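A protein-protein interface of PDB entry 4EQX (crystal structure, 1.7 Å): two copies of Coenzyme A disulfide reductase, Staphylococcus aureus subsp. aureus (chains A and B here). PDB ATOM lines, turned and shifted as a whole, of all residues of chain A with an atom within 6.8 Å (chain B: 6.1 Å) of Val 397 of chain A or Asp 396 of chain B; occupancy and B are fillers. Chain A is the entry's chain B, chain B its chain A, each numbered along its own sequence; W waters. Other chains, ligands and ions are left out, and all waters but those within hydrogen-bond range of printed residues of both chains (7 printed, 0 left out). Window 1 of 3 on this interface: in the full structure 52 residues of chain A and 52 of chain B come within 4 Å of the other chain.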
ATOM      1  N   ASN A 322     -18.820  -4.878 -33.946  1.00  0.00           N
ATOM      2  CA  ASN A 322     -17.798  -5.686 -33.226  1.00  0.00           C
ATOM      3  C   ASN A 322     -16.728  -5.987 -34.256  1.00  0.00           C
ATOM      4  O   ASN A 322     -17.047  -6.390 -35.404  1.00  0.00           O
ATOM      5  CB  ASN A 322     -18.451  -6.979 -32.638  1.00  0.00           C
ATOM      6  CG  ASN A 322     -17.597  -7.601 -31.523  1.00  0.00           C
ATOM      7  OD1 ASN A 322     -18.016  -8.540 -30.772  1.00  0.00           O
ATOM      8  ND2 ASN A 322     -16.450  -7.077 -31.378  1.00  0.00           N
ATOM      9  N   ASP A 392     -10.512 -10.510 -26.815  1.00  0.00           N
ATOM     10  CA  ASP A 392     -11.693 -11.117 -27.522  1.00  0.00           C
ATOM     11  C   ASP A 392     -12.859 -11.485 -26.529  1.00  0.00           C
ATOM     12  O   ASP A 392     -14.022 -11.263 -26.804  1.00  0.00           O
ATOM     13  CB  ASP A 392     -11.414 -12.282 -28.517  1.00  0.00           C
ATOM     14  CG  ASP A 392     -10.574 -13.382 -27.927  1.00  0.00           C
ATOM     15  OD1 ASP A 392     -10.757 -14.568 -28.301  1.00  0.00           O
ATOM     16  OD2 ASP A 392      -9.685 -13.072 -27.125  1.00  0.00           O
ATOM     17  N   LYS A 393     -12.495 -12.136 -25.445  1.00  0.00           N
ATOM     18  CA  LYS A 393     -13.493 -12.582 -24.496  1.00  0.00           C
ATOM     19  C   LYS A 393     -14.219 -11.354 -23.952  1.00  0.00           C
ATOM     20  O   LYS A 393     -15.456 -11.360 -23.889  1.00  0.00           O
ATOM     21  CB  LYS A 393     -12.824 -13.292 -23.340  1.00  0.00           C
ATOM     22  CG  LYS A 393     -13.933 -13.684 -22.254  1.00  0.00           C
ATOM     23  CD  LYS A 393     -13.422 -14.947 -21.423  1.00  0.00           C
ATOM     24  CE  LYS A 393     -12.173 -14.535 -20.626  1.00  0.00           C
ATOM     25  NZ  LYS A 393     -11.756 -15.625 -19.664  1.00  0.00           N
ATOM     26  N   ARG A 394     -13.495 -10.316 -23.534  1.00  0.00           N
ATOM     27  CA  ARG A 394     -14.207  -9.196 -22.892  1.00  0.00           C
ATOM     28  C   ARG A 394     -15.068  -8.446 -23.906  1.00  0.00           C
ATOM     29  O   ARG A 394     -16.185  -8.013 -23.599  1.00  0.00           O
ATOM     30  CB  ARG A 394     -13.227  -8.150 -22.255  1.00  0.00           C
ATOM     31  CG  ARG A 394     -12.352  -8.622 -21.086  1.00  0.00           C
ATOM     32  CD  ARG A 394     -12.940  -9.751 -20.352  1.00  0.00           C
ATOM     33  NE  ARG A 394     -12.186 -10.183 -19.144  1.00  0.00           N
ATOM     34  CZ  ARG A 394     -11.135 -11.047 -19.197  1.00  0.00           C
ATOM     35  NH1 ARG A 394     -10.638 -11.534 -18.063  1.00  0.00           N
ATOM     36  NH2 ARG A 394     -10.605 -11.434 -20.340  1.00  0.00           N
ATOM     37  N   ILE A 395     -14.547  -8.283 -25.119  1.00  0.00           N
ATOM     38  CA  ILE A 395     -15.372  -7.588 -26.128  1.00  0.00           C
ATOM     39  C   ILE A 395     -16.614  -8.362 -26.606  1.00  0.00           C
ATOM     40  O   ILE A 395     -17.692  -7.760 -26.706  1.00  0.00           O
ATOM     41  CB  ILE A 395     -14.545  -7.102 -27.309  1.00  0.00           C
ATOM     42  CG1 ILE A 395     -13.522  -6.094 -26.793  1.00  0.00           C
ATOM     43  CG2 ILE A 395     -15.472  -6.297 -28.310  1.00  0.00           C
ATOM     44  CD1 ILE A 395     -14.209  -4.767 -26.241  1.00  0.00           C
ATOM     45  N   ASP A 396     -16.513  -9.694 -26.793  1.00  0.00           N
ATOM     46  CA  ASP A 396     -17.762 -10.440 -27.052  1.00  0.00           C
ATOM     47  C   ASP A 396     -18.806 -10.366 -25.897  1.00  0.00           C
ATOM     48  O   ASP A 396     -20.008 -10.299 -26.117  1.00  0.00           O
ATOM     49  CB  ASP A 396     -17.352 -11.919 -27.345  1.00  0.00           C
ATOM     50  CG  ASP A 396     -16.874 -12.136 -28.779  1.00  0.00           C
ATOM     51  OD1 ASP A 396     -16.982 -11.241 -29.634  1.00  0.00           O
ATOM     52  OD2 ASP A 396     -16.374 -13.309 -29.031  1.00  0.00           O
ATOM     53  N   VAL A 397     -18.323 -10.417 -24.628  1.00  0.00           N
ATOM     54  CA  VAL A 397     -19.276 -10.308 -23.511  1.00  0.00           C
ATOM     55  C   VAL A 397     -19.929  -8.903 -23.579  1.00  0.00           C
ATOM     56  O   VAL A 397     -21.137  -8.785 -23.429  1.00  0.00           O
ATOM     57  CB  VAL A 397     -18.579 -10.459 -22.136  1.00  0.00           C
ATOM     58  CG1 VAL A 397     -19.580 -10.072 -21.031  1.00  0.00           C
ATOM     59  CG2 VAL A 397     -18.068 -11.935 -22.068  1.00  0.00           C
ATOM     60  N   LEU A 398     -19.137  -7.868 -23.898  1.00  0.00           N
ATOM     61  CA  LEU A 398     -19.758  -6.558 -23.952  1.00  0.00           C
ATOM     62  C   LEU A 398     -20.644  -6.377 -25.209  1.00  0.00           C
ATOM     63  O   LEU A 398     -21.668  -5.647 -25.071  1.00  0.00           O
ATOM     64  CB  LEU A 398     -18.713  -5.474 -23.860  1.00  0.00           C
ATOM     65  CG  LEU A 398     -18.082  -5.438 -22.447  1.00  0.00           C
ATOM     66  CD1 LEU A 398     -16.802  -4.652 -22.466  1.00  0.00           C
ATOM     67  CD2 LEU A 398     -19.022  -4.726 -21.463  1.00  0.00           C
ATOM     68  N   SER A 399     -20.283  -7.027 -26.329  1.00  0.00           N
ATOM     69  CA  SER A 399     -21.238  -7.088 -27.474  1.00  0.00           C
ATOM     70  C   SER A 399     -22.611  -7.629 -27.006  1.00  0.00           C
ATOM     71  O   SER A 399     -23.735  -7.014 -27.237  1.00  0.00           O
ATOM     72  CB  SER A 399     -20.669  -7.909 -28.630  1.00  0.00           C
ATOM     73  OG  SER A 399     -21.633  -7.914 -29.694  1.00  0.00           O
ATOM     74  N   MET A 400     -22.574  -8.735 -26.236  1.00  0.00           N
ATOM     75  CA  MET A 400     -23.842  -9.333 -25.699  1.00  0.00           C
ATOM     76  C   MET A 400     -24.561  -8.389 -24.678  1.00  0.00           C
ATOM     77  O   MET A 400     -25.847  -8.296 -24.686  1.00  0.00           O
ATOM     78  CB  MET A 400     -23.555 -10.744 -25.136  1.00  0.00           C
ATOM     79  CG  MET A 400     -24.833 -11.383 -24.484  1.00  0.00           C
ATOM     80  SD  MET A 400     -26.096 -11.769 -25.714  1.00  0.00           S
ATOM     81  CE  MET A 400     -25.329 -13.213 -26.413  1.00  0.00           C
ATOM     82  N   ALA A 401     -23.797  -7.678 -23.838  1.00  0.00           N
ATOM     83  CA  ALA A 401     -24.418  -6.694 -22.987  1.00  0.00           C
ATOM     84  C   ALA A 401     -25.086  -5.616 -23.777  1.00  0.00           C
ATOM     85  O   ALA A 401     -26.181  -5.201 -23.389  1.00  0.00           O
ATOM     86  CB  ALA A 401     -23.313  -6.052 -22.116  1.00  0.00           C
ATOM     87  N   MET A 402     -24.423  -5.087 -24.812  1.00  0.00           N
ATOM     88  CA  MET A 402     -25.059  -3.985 -25.606  1.00  0.00           C
ATOM     89  C   MET A 402     -26.288  -4.494 -26.355  1.00  0.00           C
ATOM     90  O   MET A 402     -27.231  -3.740 -26.518  1.00  0.00           O
ATOM     91  CB  MET A 402     -24.054  -3.396 -26.605  1.00  0.00           C
ATOM     92  CG  MET A 402     -22.901  -2.832 -25.800  1.00  0.00           C
ATOM     93  SD  MET A 402     -21.386  -2.423 -26.731  1.00  0.00           S
ATOM     94  CE  MET A 402     -21.931  -1.051 -27.525  1.00  0.00           C
ATOM     95  N   LEU A 411     -22.898  -3.750 -15.067  1.00  0.00           N
ATOM     96  CA  LEU A 411     -21.719  -4.619 -15.327  1.00  0.00           C
ATOM     97  C   LEU A 411     -21.119  -5.184 -14.002  1.00  0.00           C
ATOM     98  O   LEU A 411     -20.442  -6.188 -14.030  1.00  0.00           O
ATOM     99  CB  LEU A 411     -20.603  -3.913 -16.098  1.00  0.00           C
ATOM    100  CG  LEU A 411     -20.990  -3.549 -17.534  1.00  0.00           C
ATOM    101  CD1 LEU A 411     -19.906  -2.611 -18.138  1.00  0.00           C
ATOM    102  CD2 LEU A 411     -21.151  -4.917 -18.359  1.00  0.00           C
ATOM    103  N   PHE A 414     -22.384  -8.849 -13.714  1.00  0.00           N
ATOM    104  CA  PHE A 414     -21.940  -9.853 -14.648  1.00  0.00           C
ATOM    105  C   PHE A 414     -21.224 -10.949 -13.880  1.00  0.00           C
ATOM    106  O   PHE A 414     -20.228 -10.728 -13.191  1.00  0.00           O
ATOM    107  CB  PHE A 414     -20.981  -9.225 -15.682  1.00  0.00           C
ATOM    108  CG  PHE A 414     -20.153 -10.248 -16.459  1.00  0.00           C
ATOM    109  CD1 PHE A 414     -20.726 -11.256 -17.214  1.00  0.00           C
ATOM    110  CD2 PHE A 414     -18.806 -10.211 -16.342  1.00  0.00           C
ATOM    111  CE1 PHE A 414     -19.840 -12.255 -17.922  1.00  0.00           C
ATOM    112  CE2 PHE A 414     -17.961 -11.158 -17.021  1.00  0.00           C
ATOM    113  CZ  PHE A 414     -18.506 -12.153 -17.858  1.00  0.00           C
ATOM    114  N   GLU A 415     -21.727 -12.165 -14.033  1.00  0.00           N
ATOM    115  CA  GLU A 415     -21.120 -13.320 -13.285  1.00  0.00           C
ATOM    116  C   GLU A 415     -20.163 -14.074 -14.198  1.00  0.00           C
ATOM    117  O   GLU A 415     -20.550 -14.931 -15.030  1.00  0.00           O
ATOM    118  CB  GLU A 415     -22.217 -14.251 -12.746  1.00  0.00           C
ATOM    119  CG  GLU A 415     -21.718 -15.409 -11.839  1.00  0.00           C
ATOM    120  CD  GLU A 415     -22.873 -16.257 -11.276  1.00  0.00           C
ATOM    121  OE1 GLU A 415     -22.632 -17.474 -10.953  1.00  0.00           O
ATOM    122  OE2 GLU A 415     -24.003 -15.640 -11.004  1.00  0.00           O
ATOM    123  N   VAL A 416     -18.865 -13.765 -14.030  1.00  0.00           N
ATOM    124  CA  VAL A 416     -17.788 -14.343 -14.814  1.00  0.00           C
ATOM    125  C   VAL A 416     -17.495 -15.779 -14.383  1.00  0.00           C
ATOM    126  O   VAL A 416     -17.749 -16.182 -13.243  1.00  0.00           O
ATOM    127  CB  VAL A 416     -16.494 -13.476 -14.654  1.00  0.00           C
ATOM    128  CG1 VAL A 416     -15.791 -13.671 -13.237  1.00  0.00           C
ATOM    129  CG2 VAL A 416     -15.433 -13.670 -15.843  1.00  0.00           C
ATOM    130  N   ALA A 417     -16.921 -16.532 -15.314  1.00  0.00           N
ATOM    131  CA  ALA A 417     -16.344 -17.833 -15.034  1.00  0.00           C
ATOM    132  C   ALA A 417     -14.926 -17.604 -14.503  1.00  0.00           C
ATOM    133  O   ALA A 417     -14.007 -17.222 -15.279  1.00  0.00           O
ATOM    134  CB  ALA A 417     -16.271 -18.702 -16.311  1.00  0.00           C
ATOM    135  N   TYR A 418     -14.779 -17.840 -13.187  1.00  0.00           N
ATOM    136  CA  TYR A 418     -13.509 -17.594 -12.508  1.00  0.00           C
ATOM    137  C   TYR A 418     -12.819 -18.885 -12.038  1.00  0.00           C
ATOM    138  O   TYR A 418     -13.360 -19.660 -11.246  1.00  0.00           O
ATOM    139  CB  TYR A 418     -13.621 -16.660 -11.293  1.00  0.00           C
ATOM    140  CG  TYR A 418     -12.315 -16.700 -10.575  1.00  0.00           C
ATOM    141  CD1 TYR A 418     -11.187 -16.090 -11.165  1.00  0.00           C
ATOM    142  CD2 TYR A 418     -12.218 -17.305  -9.284  1.00  0.00           C
ATOM    143  CE1 TYR A 418      -9.913 -16.113 -10.537  1.00  0.00           C
ATOM    144  CE2 TYR A 418     -10.948 -17.302  -8.622  1.00  0.00           C
ATOM    145  CZ  TYR A 418      -9.804 -16.711  -9.288  1.00  0.00           C
ATOM    146  OH  TYR A 418      -8.515 -16.704  -8.723  1.00  0.00           O
ATOM    147  N   TYR A 422      -8.115 -17.913 -15.927  1.00  0.00           N
ATOM    148  CA  TYR A 422      -9.100 -17.320 -16.828  1.00  0.00           C
ATOM    149  C   TYR A 422      -9.500 -15.873 -16.549  1.00  0.00           C
ATOM    150  O   TYR A 422      -9.889 -15.159 -17.485  1.00  0.00           O
ATOM    151  CB  TYR A 422     -10.408 -18.150 -16.837  1.00  0.00           C
ATOM    152  CG  TYR A 422     -10.134 -19.620 -17.225  1.00  0.00           C
ATOM    153  CD1 TYR A 422     -10.076 -20.600 -16.262  1.00  0.00           C
ATOM    154  CD2 TYR A 422      -9.756 -19.957 -18.560  1.00  0.00           C
ATOM    155  CE1 TYR A 422      -9.792 -21.974 -16.595  1.00  0.00           C
ATOM    156  CE2 TYR A 422      -9.543 -21.321 -18.935  1.00  0.00           C
ATOM    157  CZ  TYR A 422      -9.471 -22.272 -17.960  1.00  0.00           C
ATOM    158  OH  TYR A 422      -9.202 -23.549 -18.333  1.00  0.00           O
ATOM    159  N   SER A 423      -9.509 -15.470 -15.275  1.00  0.00           N
ATOM    160  CA  SER A 423     -10.074 -14.132 -14.944  1.00  0.00           C
ATOM    161  C   SER A 423      -9.729 -13.833 -13.467  1.00  0.00           C
ATOM    162  O   SER A 423      -8.709 -14.301 -12.993  1.00  0.00           O
ATOM    163  CB  SER A 423     -11.615 -14.141 -15.139  1.00  0.00           C
ATOM    164  OG  SER A 423     -12.219 -15.219 -14.329  1.00  0.00           O
ATOM    165  N   ASP A 427     -14.166  -9.486 -12.313  1.00  0.00           N
ATOM    166  CA  ASP A 427     -13.461  -9.505 -13.591  1.00  0.00           C
ATOM    167  C   ASP A 427     -13.230  -8.014 -13.949  1.00  0.00           C
ATOM    168  O   ASP A 427     -13.847  -7.076 -13.394  1.00  0.00           O
ATOM    169  CB  ASP A 427     -14.318 -10.187 -14.684  1.00  0.00           C
ATOM    170  CG  ASP A 427     -13.593 -10.199 -15.999  1.00  0.00           C
ATOM    171  OD1 ASP A 427     -14.139  -9.684 -17.012  1.00  0.00           O
ATOM    172  OD2 ASP A 427     -12.449 -10.735 -15.909  1.00  0.00           O
ATOM    173  N   ILE A 429     -14.587  -6.607 -16.473  1.00  0.00           N
ATOM    174  CA  ILE A 429     -15.856  -6.104 -16.753  1.00  0.00           C
ATOM    175  C   ILE A 429     -16.558  -5.641 -15.489  1.00  0.00           C
ATOM    176  O   ILE A 429     -17.240  -4.615 -15.500  1.00  0.00           O
ATOM    177  CB  ILE A 429     -16.687  -7.189 -17.540  1.00  0.00           C
ATOM    178  CG1 ILE A 429     -16.091  -7.339 -18.963  1.00  0.00           C
ATOM    179  CG2 ILE A 429     -18.201  -6.823 -17.529  1.00  0.00           C
ATOM    180  CD1 ILE A 429     -16.709  -8.545 -19.708  1.00  0.00           C
ATOM    181  N   ASN B 322     -22.053 -19.586 -12.795  1.00  0.00           N
ATOM    182  CA  ASN B 322     -20.955 -19.703 -13.771  1.00  0.00           C
ATOM    183  C   ASN B 322     -19.738 -20.277 -13.100  1.00  0.00           C
ATOM    184  O   ASN B 322     -19.374 -19.860 -11.986  1.00  0.00           O
ATOM    185  CB  ASN B 322     -20.642 -18.310 -14.336  1.00  0.00           C
ATOM    186  CG  ASN B 322     -19.942 -18.341 -15.697  1.00  0.00           C
ATOM    187  OD1 ASN B 322     -19.765 -17.217 -16.347  1.00  0.00           O
ATOM    188  ND2 ASN B 322     -19.517 -19.520 -16.128  1.00  0.00           N
ATOM    189  N   ALA B 391     -13.703 -22.165 -24.732  1.00  0.00           N
ATOM    190  CA  ALA B 391     -14.814 -22.484 -23.833  1.00  0.00           C
ATOM    191  C   ALA B 391     -15.137 -21.365 -22.863  1.00  0.00           C
ATOM    192  O   ALA B 391     -16.323 -21.098 -22.633  1.00  0.00           O
ATOM    193  CB  ALA B 391     -14.571 -23.814 -23.058  1.00  0.00           C
ATOM    194  N   ASP B 392     -14.132 -20.724 -22.259  1.00  0.00           N
ATOM    195  CA  ASP B 392     -14.461 -19.710 -21.261  1.00  0.00           C
ATOM    196  C   ASP B 392     -15.114 -18.519 -22.007  1.00  0.00           C
ATOM    197  O   ASP B 392     -16.003 -17.871 -21.451  1.00  0.00           O
ATOM    198  CB  ASP B 392     -13.192 -19.241 -20.513  1.00  0.00           C
ATOM    199  CG  ASP B 392     -11.999 -18.945 -21.479  1.00  0.00           C
ATOM    200  OD1 ASP B 392     -11.298 -17.937 -21.277  1.00  0.00           O
ATOM    201  OD2 ASP B 392     -11.730 -19.712 -22.472  1.00  0.00           O
ATOM    202  N   LYS B 393     -14.655 -18.228 -23.228  1.00  0.00           N
ATOM    203  CA  LYS B 393     -15.277 -17.060 -23.971  1.00  0.00           C
ATOM    204  C   LYS B 393     -16.800 -17.322 -24.266  1.00  0.00           C
ATOM    205  O   LYS B 393     -17.674 -16.455 -23.979  1.00  0.00           O
ATOM    206  CB  LYS B 393     -14.530 -16.828 -25.348  1.00  0.00           C
ATOM    207  CG  LYS B 393     -15.219 -15.719 -26.149  1.00  0.00           C
ATOM    208  CD  LYS B 393     -14.191 -15.160 -27.190  1.00  0.00           C
ATOM    209  CE  LYS B 393     -13.979 -16.190 -28.319  1.00  0.00           C
ATOM    210  NZ  LYS B 393     -13.043 -15.591 -29.378  1.00  0.00           N
ATOM    211  N   ARG B 394     -17.130 -18.525 -24.706  1.00  0.00           N
ATOM    212  CA  ARG B 394     -18.552 -18.767 -25.065  1.00  0.00           C
ATOM    213  C   ARG B 394     -19.386 -18.787 -23.785  1.00  0.00           C
ATOM    214  O   ARG B 394     -20.548 -18.389 -23.816  1.00  0.00           O
ATOM    215  CB  ARG B 394     -18.707 -20.112 -25.724  1.00  0.00           C
ATOM    216  CG  ARG B 394     -17.915 -20.286 -27.062  1.00  0.00           C
ATOM    217  CD  ARG B 394     -17.791 -19.005 -27.866  1.00  0.00           C
ATOM    218  NE  ARG B 394     -17.249 -19.123 -29.266  1.00  0.00           N
ATOM    219  CZ  ARG B 394     -15.960 -19.278 -29.583  1.00  0.00           C
ATOM    220  NH1 ARG B 394     -15.607 -19.229 -30.886  1.00  0.00           N
ATOM    221  NH2 ARG B 394     -15.030 -19.538 -28.672  1.00  0.00           N
ATOM    222  N   ILE B 395     -18.806 -19.333 -22.711  1.00  0.00           N
ATOM    223  CA  ILE B 395     -19.637 -19.479 -21.508  1.00  0.00           C
ATOM    224  C   ILE B 395     -19.877 -18.120 -20.836  1.00  0.00           C
ATOM    225  O   ILE B 395     -20.993 -17.816 -20.327  1.00  0.00           O
ATOM    226  CB  ILE B 395     -19.097 -20.590 -20.541  1.00  0.00           C
ATOM    227  CG1 ILE B 395     -19.279 -21.969 -21.187  1.00  0.00           C
ATOM    228  CG2 ILE B 395     -19.869 -20.569 -19.201  1.00  0.00           C
ATOM    229  CD1 ILE B 395     -20.860 -22.355 -21.529  1.00  0.00           C
ATOM    230  N   ASP B 396     -18.852 -17.301 -20.859  1.00  0.00           N
ATOM    231  CA  ASP B 396     -19.037 -15.930 -20.327  1.00  0.00           C
ATOM    232  C   ASP B 396     -20.074 -15.159 -21.168  1.00  0.00           C
ATOM    233  O   ASP B 396     -20.905 -14.377 -20.623  1.00  0.00           O
ATOM    234  CB  ASP B 396     -17.740 -15.081 -20.269  1.00  0.00           C
ATOM    235  CG  ASP B 396     -16.871 -15.406 -18.986  1.00  0.00           C
ATOM    236  OD1 ASP B 396     -17.472 -16.019 -18.063  1.00  0.00           O
ATOM    237  OD2 ASP B 396     -15.712 -14.898 -18.907  1.00  0.00           O
ATOM    238  N   VAL B 397     -20.057 -15.369 -22.507  1.00  0.00           N
ATOM    239  CA  VAL B 397     -21.063 -14.664 -23.338  1.00  0.00           C
ATOM    240  C   VAL B 397     -22.481 -15.147 -22.922  1.00  0.00           C
ATOM    241  O   VAL B 397     -23.388 -14.378 -22.855  1.00  0.00           O
ATOM    242  CB  VAL B 397     -20.787 -14.828 -24.885  1.00  0.00           C
ATOM    243  CG1 VAL B 397     -21.888 -14.273 -25.758  1.00  0.00           C
ATOM    244  CG2 VAL B 397     -19.497 -14.113 -25.297  1.00  0.00           C
ATOM    245  N   LEU B 398     -22.639 -16.414 -22.701  1.00  0.00           N
ATOM    246  CA  LEU B 398     -23.941 -16.964 -22.428  1.00  0.00           C
ATOM    247  C   LEU B 398     -24.369 -16.607 -20.993  1.00  0.00           C
ATOM    248  O   LEU B 398     -25.560 -16.423 -20.730  1.00  0.00           O
ATOM    249  CB  LEU B 398     -23.876 -18.485 -22.655  1.00  0.00           C
ATOM    250  CG  LEU B 398     -23.845 -18.786 -24.216  1.00  0.00           C
ATOM    251  CD1 LEU B 398     -23.518 -20.210 -24.522  1.00  0.00           C
ATOM    252  CD2 LEU B 398     -25.263 -18.494 -24.788  1.00  0.00           C
ATOM    253  N   SER B 399     -23.397 -16.465 -20.057  1.00  0.00           N
ATOM    254  CA  SER B 399     -23.792 -15.932 -18.753  1.00  0.00           C
ATOM    255  C   SER B 399     -24.388 -14.487 -18.905  1.00  0.00           C
ATOM    256  O   SER B 399     -25.457 -14.197 -18.344  1.00  0.00           O
ATOM    257  CB  SER B 399     -22.518 -15.899 -17.861  1.00  0.00           C
ATOM    258  OG  SER B 399     -22.888 -15.259 -16.649  1.00  0.00           O
ATOM    259  N   MET B 400     -23.747 -13.627 -19.738  1.00  0.00           N
ATOM    260  CA  MET B 400     -24.273 -12.329 -20.008  1.00  0.00           C
ATOM    261  C   MET B 400     -25.696 -12.427 -20.650  1.00  0.00           C
ATOM    262  O   MET B 400     -26.582 -11.599 -20.393  1.00  0.00           O
ATOM    263  CB  MET B 400     -23.255 -11.490 -20.779  1.00  0.00           C
ATOM    264  CG  MET B 400     -23.808 -10.121 -21.291  1.00  0.00           C
ATOM    265  SD  MET B 400     -24.187  -9.056 -19.835  1.00  0.00           S
ATOM    266  CE  MET B 400     -22.576  -8.640 -19.216  1.00  0.00           C
ATOM    267  N   ALA B 401     -25.859 -13.394 -21.564  1.00  0.00           N
ATOM    268  CA  ALA B 401     -27.159 -13.576 -22.219  1.00  0.00           C
ATOM    269  C   ALA B 401     -28.228 -14.011 -21.189  1.00  0.00           C
ATOM    270  O   ALA B 401     -29.329 -13.473 -21.195  1.00  0.00           O
ATOM    271  CB  ALA B 401     -26.979 -14.591 -23.278  1.00  0.00           C
ATOM    272  N   PHE B 414     -26.377 -12.605 -32.016  1.00  0.00           N
ATOM    273  CA  PHE B 414     -25.171 -12.228 -31.321  1.00  0.00           C
ATOM    274  C   PHE B 414     -24.066 -11.826 -32.308  1.00  0.00           C
ATOM    275  O   PHE B 414     -23.748 -12.592 -33.199  1.00  0.00           O
ATOM    276  CB  PHE B 414     -24.716 -13.424 -30.408  1.00  0.00           C
ATOM    277  CG  PHE B 414     -23.252 -13.346 -29.991  1.00  0.00           C
ATOM    278  CD1 PHE B 414     -22.850 -12.276 -29.193  1.00  0.00           C
ATOM    279  CD2 PHE B 414     -22.337 -14.308 -30.364  1.00  0.00           C
ATOM    280  CE1 PHE B 414     -21.507 -12.205 -28.742  1.00  0.00           C
ATOM    281  CE2 PHE B 414     -20.991 -14.269 -29.975  1.00  0.00           C
ATOM    282  CZ  PHE B 414     -20.555 -13.177 -29.184  1.00  0.00           C
HETATM  283  O   HOH W   1     -13.731 -16.320 -17.884  1.00  0.00           O
HETATM  284  O   HOH W   2     -14.317 -13.628 -30.620  1.00  0.00           O
HETATM  285  O   HOH W   3     -20.312 -17.981  -9.584  1.00  0.00           O
HETATM  286  O   HOH W   4     -14.595 -12.391 -19.123  1.00  0.00           O
HETATM  287  O   HOH W   5     -23.807 -12.678 -15.878  1.00  0.00           O
HETATM  288  O   HOH W   6     -17.471 -15.832 -28.881  1.00  0.00           O
HETATM  289  O   HOH W   7     -17.238 -18.202 -11.491  1.00  0.00           O
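Asp 392 of chain A touches Lys 393 of chain B, and with the chains exchanged Lys 393 of chain A touches Asp 392 of chain B. Lys 393 of chain B touches its own counterpart, Lys 393 of chain A. Asp 396 of chain A touches Phe 414 of chain B, and with the chains exchanged Phe 414 of chain A touches Asp 396 of chain B. Val 397 of chain A touches its own counterpart, Val 397 of chain B.
Water W1 lies within hydrogen-bond range of OD2 of Asp 396 of chain B (2.6 Å), NZ of Lys 393 of chain A (2.7 Å) and O of Ala 417 of chain A (2.8 Å). Water W7 lies within hydrogen-bond range of O of Val 416 of chain A, O of Asn 322 of chain B and N of Tyr 418 of chain A. Water W3 lies within hydrogen-bond range of OE1 of Glu 415 of chain A (2.7 Å) and O of Asn 322 of chain B (3.2 Å). Water W4 lies within hydrogen-bond range of the side-chain carboxylate (OD2) of Asp 396 of chain B (2.8 Å), the guanidinium group (NE) of Arg 394 of chain A (3.3 Å) and the side-chain carboxylate (OD1) of Asp 427 of chain A (3.5 Å). Water W6 bridges the side-chain carboxylate of Asp 396 of chain A (2.8 Å) and the guanidinium group of Arg 394 of chain B (3.3 Å). Water W5 bridges the backbone NH (N) of Glu 415 of chain A (2.8 Å) and the side-chain hydroxyl (OG) of Ser 399 of chain B (2.8 Å).
Among the printed residues, pairs that only touch across the chains: Lys 393 of chain A with Lys 393 of chain B (3.8 Å), Lys 393 of chain A with Asp 396 of chain B (3.4 Å), Asp 396 of chain A with Lys 393 of chain B (3.4 Å), Asp 396 of chain A with Val 397 of chain B (3.7 Å), Asp 396 of chain A with Phe 414 of chain B (3.6 Å), Val 397 of chain A with Asp 396 of chain B (3.6 Å), Val 397 of chain A with Val 397 of chain B (3.9 Å), Val 397 of chain A with Met 400 of chain B (3.7 Å), Met 400 of chain A with Val 397 of chain B (3.7 Å), Met 400 of chain A with Met 400 of chain B (3.6 Å), Met 400 of chain A with Ala 401 of chain B (3.7 Å), Met 400 of chain A with Phe 414 of chain B (3.8 Å), Ala 401 of chain A with Met 400 of chain B (3.5 Å), Phe 414 of chain A with Asp 396 of chain B (3.6 Å), Phe 414 of chain A with Met 400 of chain B (3.8 Å), Val 416 of chain A with Asn 322 of chain B (3.3 Å), Val 416 of chain A with Asp 396 of chain B (3.3 Å) and Tyr 422 of chain A with Asp 392 of chain B (3.7 Å).
The backbone carbonyl oxygen (O) of Glu 415 of chain A lies close to the side-chain amide oxygen (OD1) of Asn 322 of chain B. The side-chain amide oxygen of Asn 322 of chain B lies within hydrogen-bond range of the backbone NH of Ala 417 of chain A. The side-chain amino group (NZ) of Lys 393 of chain A is in salt-bridge range of the side-chain carboxylate (OD1) of Asp 392 of chain B, at 2.9 Å. The side-chain amino group (NZ) of Lys 393 of chain B lies within salt-bridge range of the side-chain carboxylate (OD1) of Asp 392 of chain A (2.7 Å). N of Ala 417 of chain A sits at hydrogen-bond distance from OD1 of Asp 396 of chain B (2.9 Å). O of Glu 415 of chain A lies within hydrogen-bond range of OG of Ser 399 of chain B, at 2.9 Å.
Of chain B, only Asp 396 (3.6 Å), Val 397 (3.9 Å) and Met 400 (3.7 Å) come within 4 Å of Val 397 of chain A. Asp 396 of chain B touches just these residues of chain A: Lys 393 (3.4 Å), Val 397 (3.6 Å), Phe 414 (3.6 Å), Val 416 (3.3 Å) and Ala 417 (2.9 Å). Printed residues of chain B within 4 Å of Glu 415 of chain A: Asn 322 and Ser 399. Of the printed residues of chain A, Asp 392 of chain B touches Lys 393 and Tyr 422. Met 402 of chain A touches none of the printed residues of chain B. The nearest printed residue of chain B that does not touch Ala 401 of chain A is Ala 401 of chain B (6.5 Å).
Of the 13 printed residues of chain B, 9 touch a printed residue of chain A. Hydrophobic or aromatic side chains of chain A within 4 Å of the printed part of chain B: Val 397, Met 400, Ala 401, Phe 414, Val 416, Ala 417 and Tyr 422.
OD1 of Asn 322 of chain B lies close to OD1 of Asp 396 of chain B, 3.1 Å away. OD1 of Asn 322 of chain A sits close to OD1 of Asp 396 of chain A (3.1 Å). O of Tyr 422 of chain A lies within hydrogen-bond range of NZ of Lys 393 of chain A. O of Ala 417 of chain A lies within hydrogen-bond range of OG of Ser 423 of chain A (2.8 Å).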
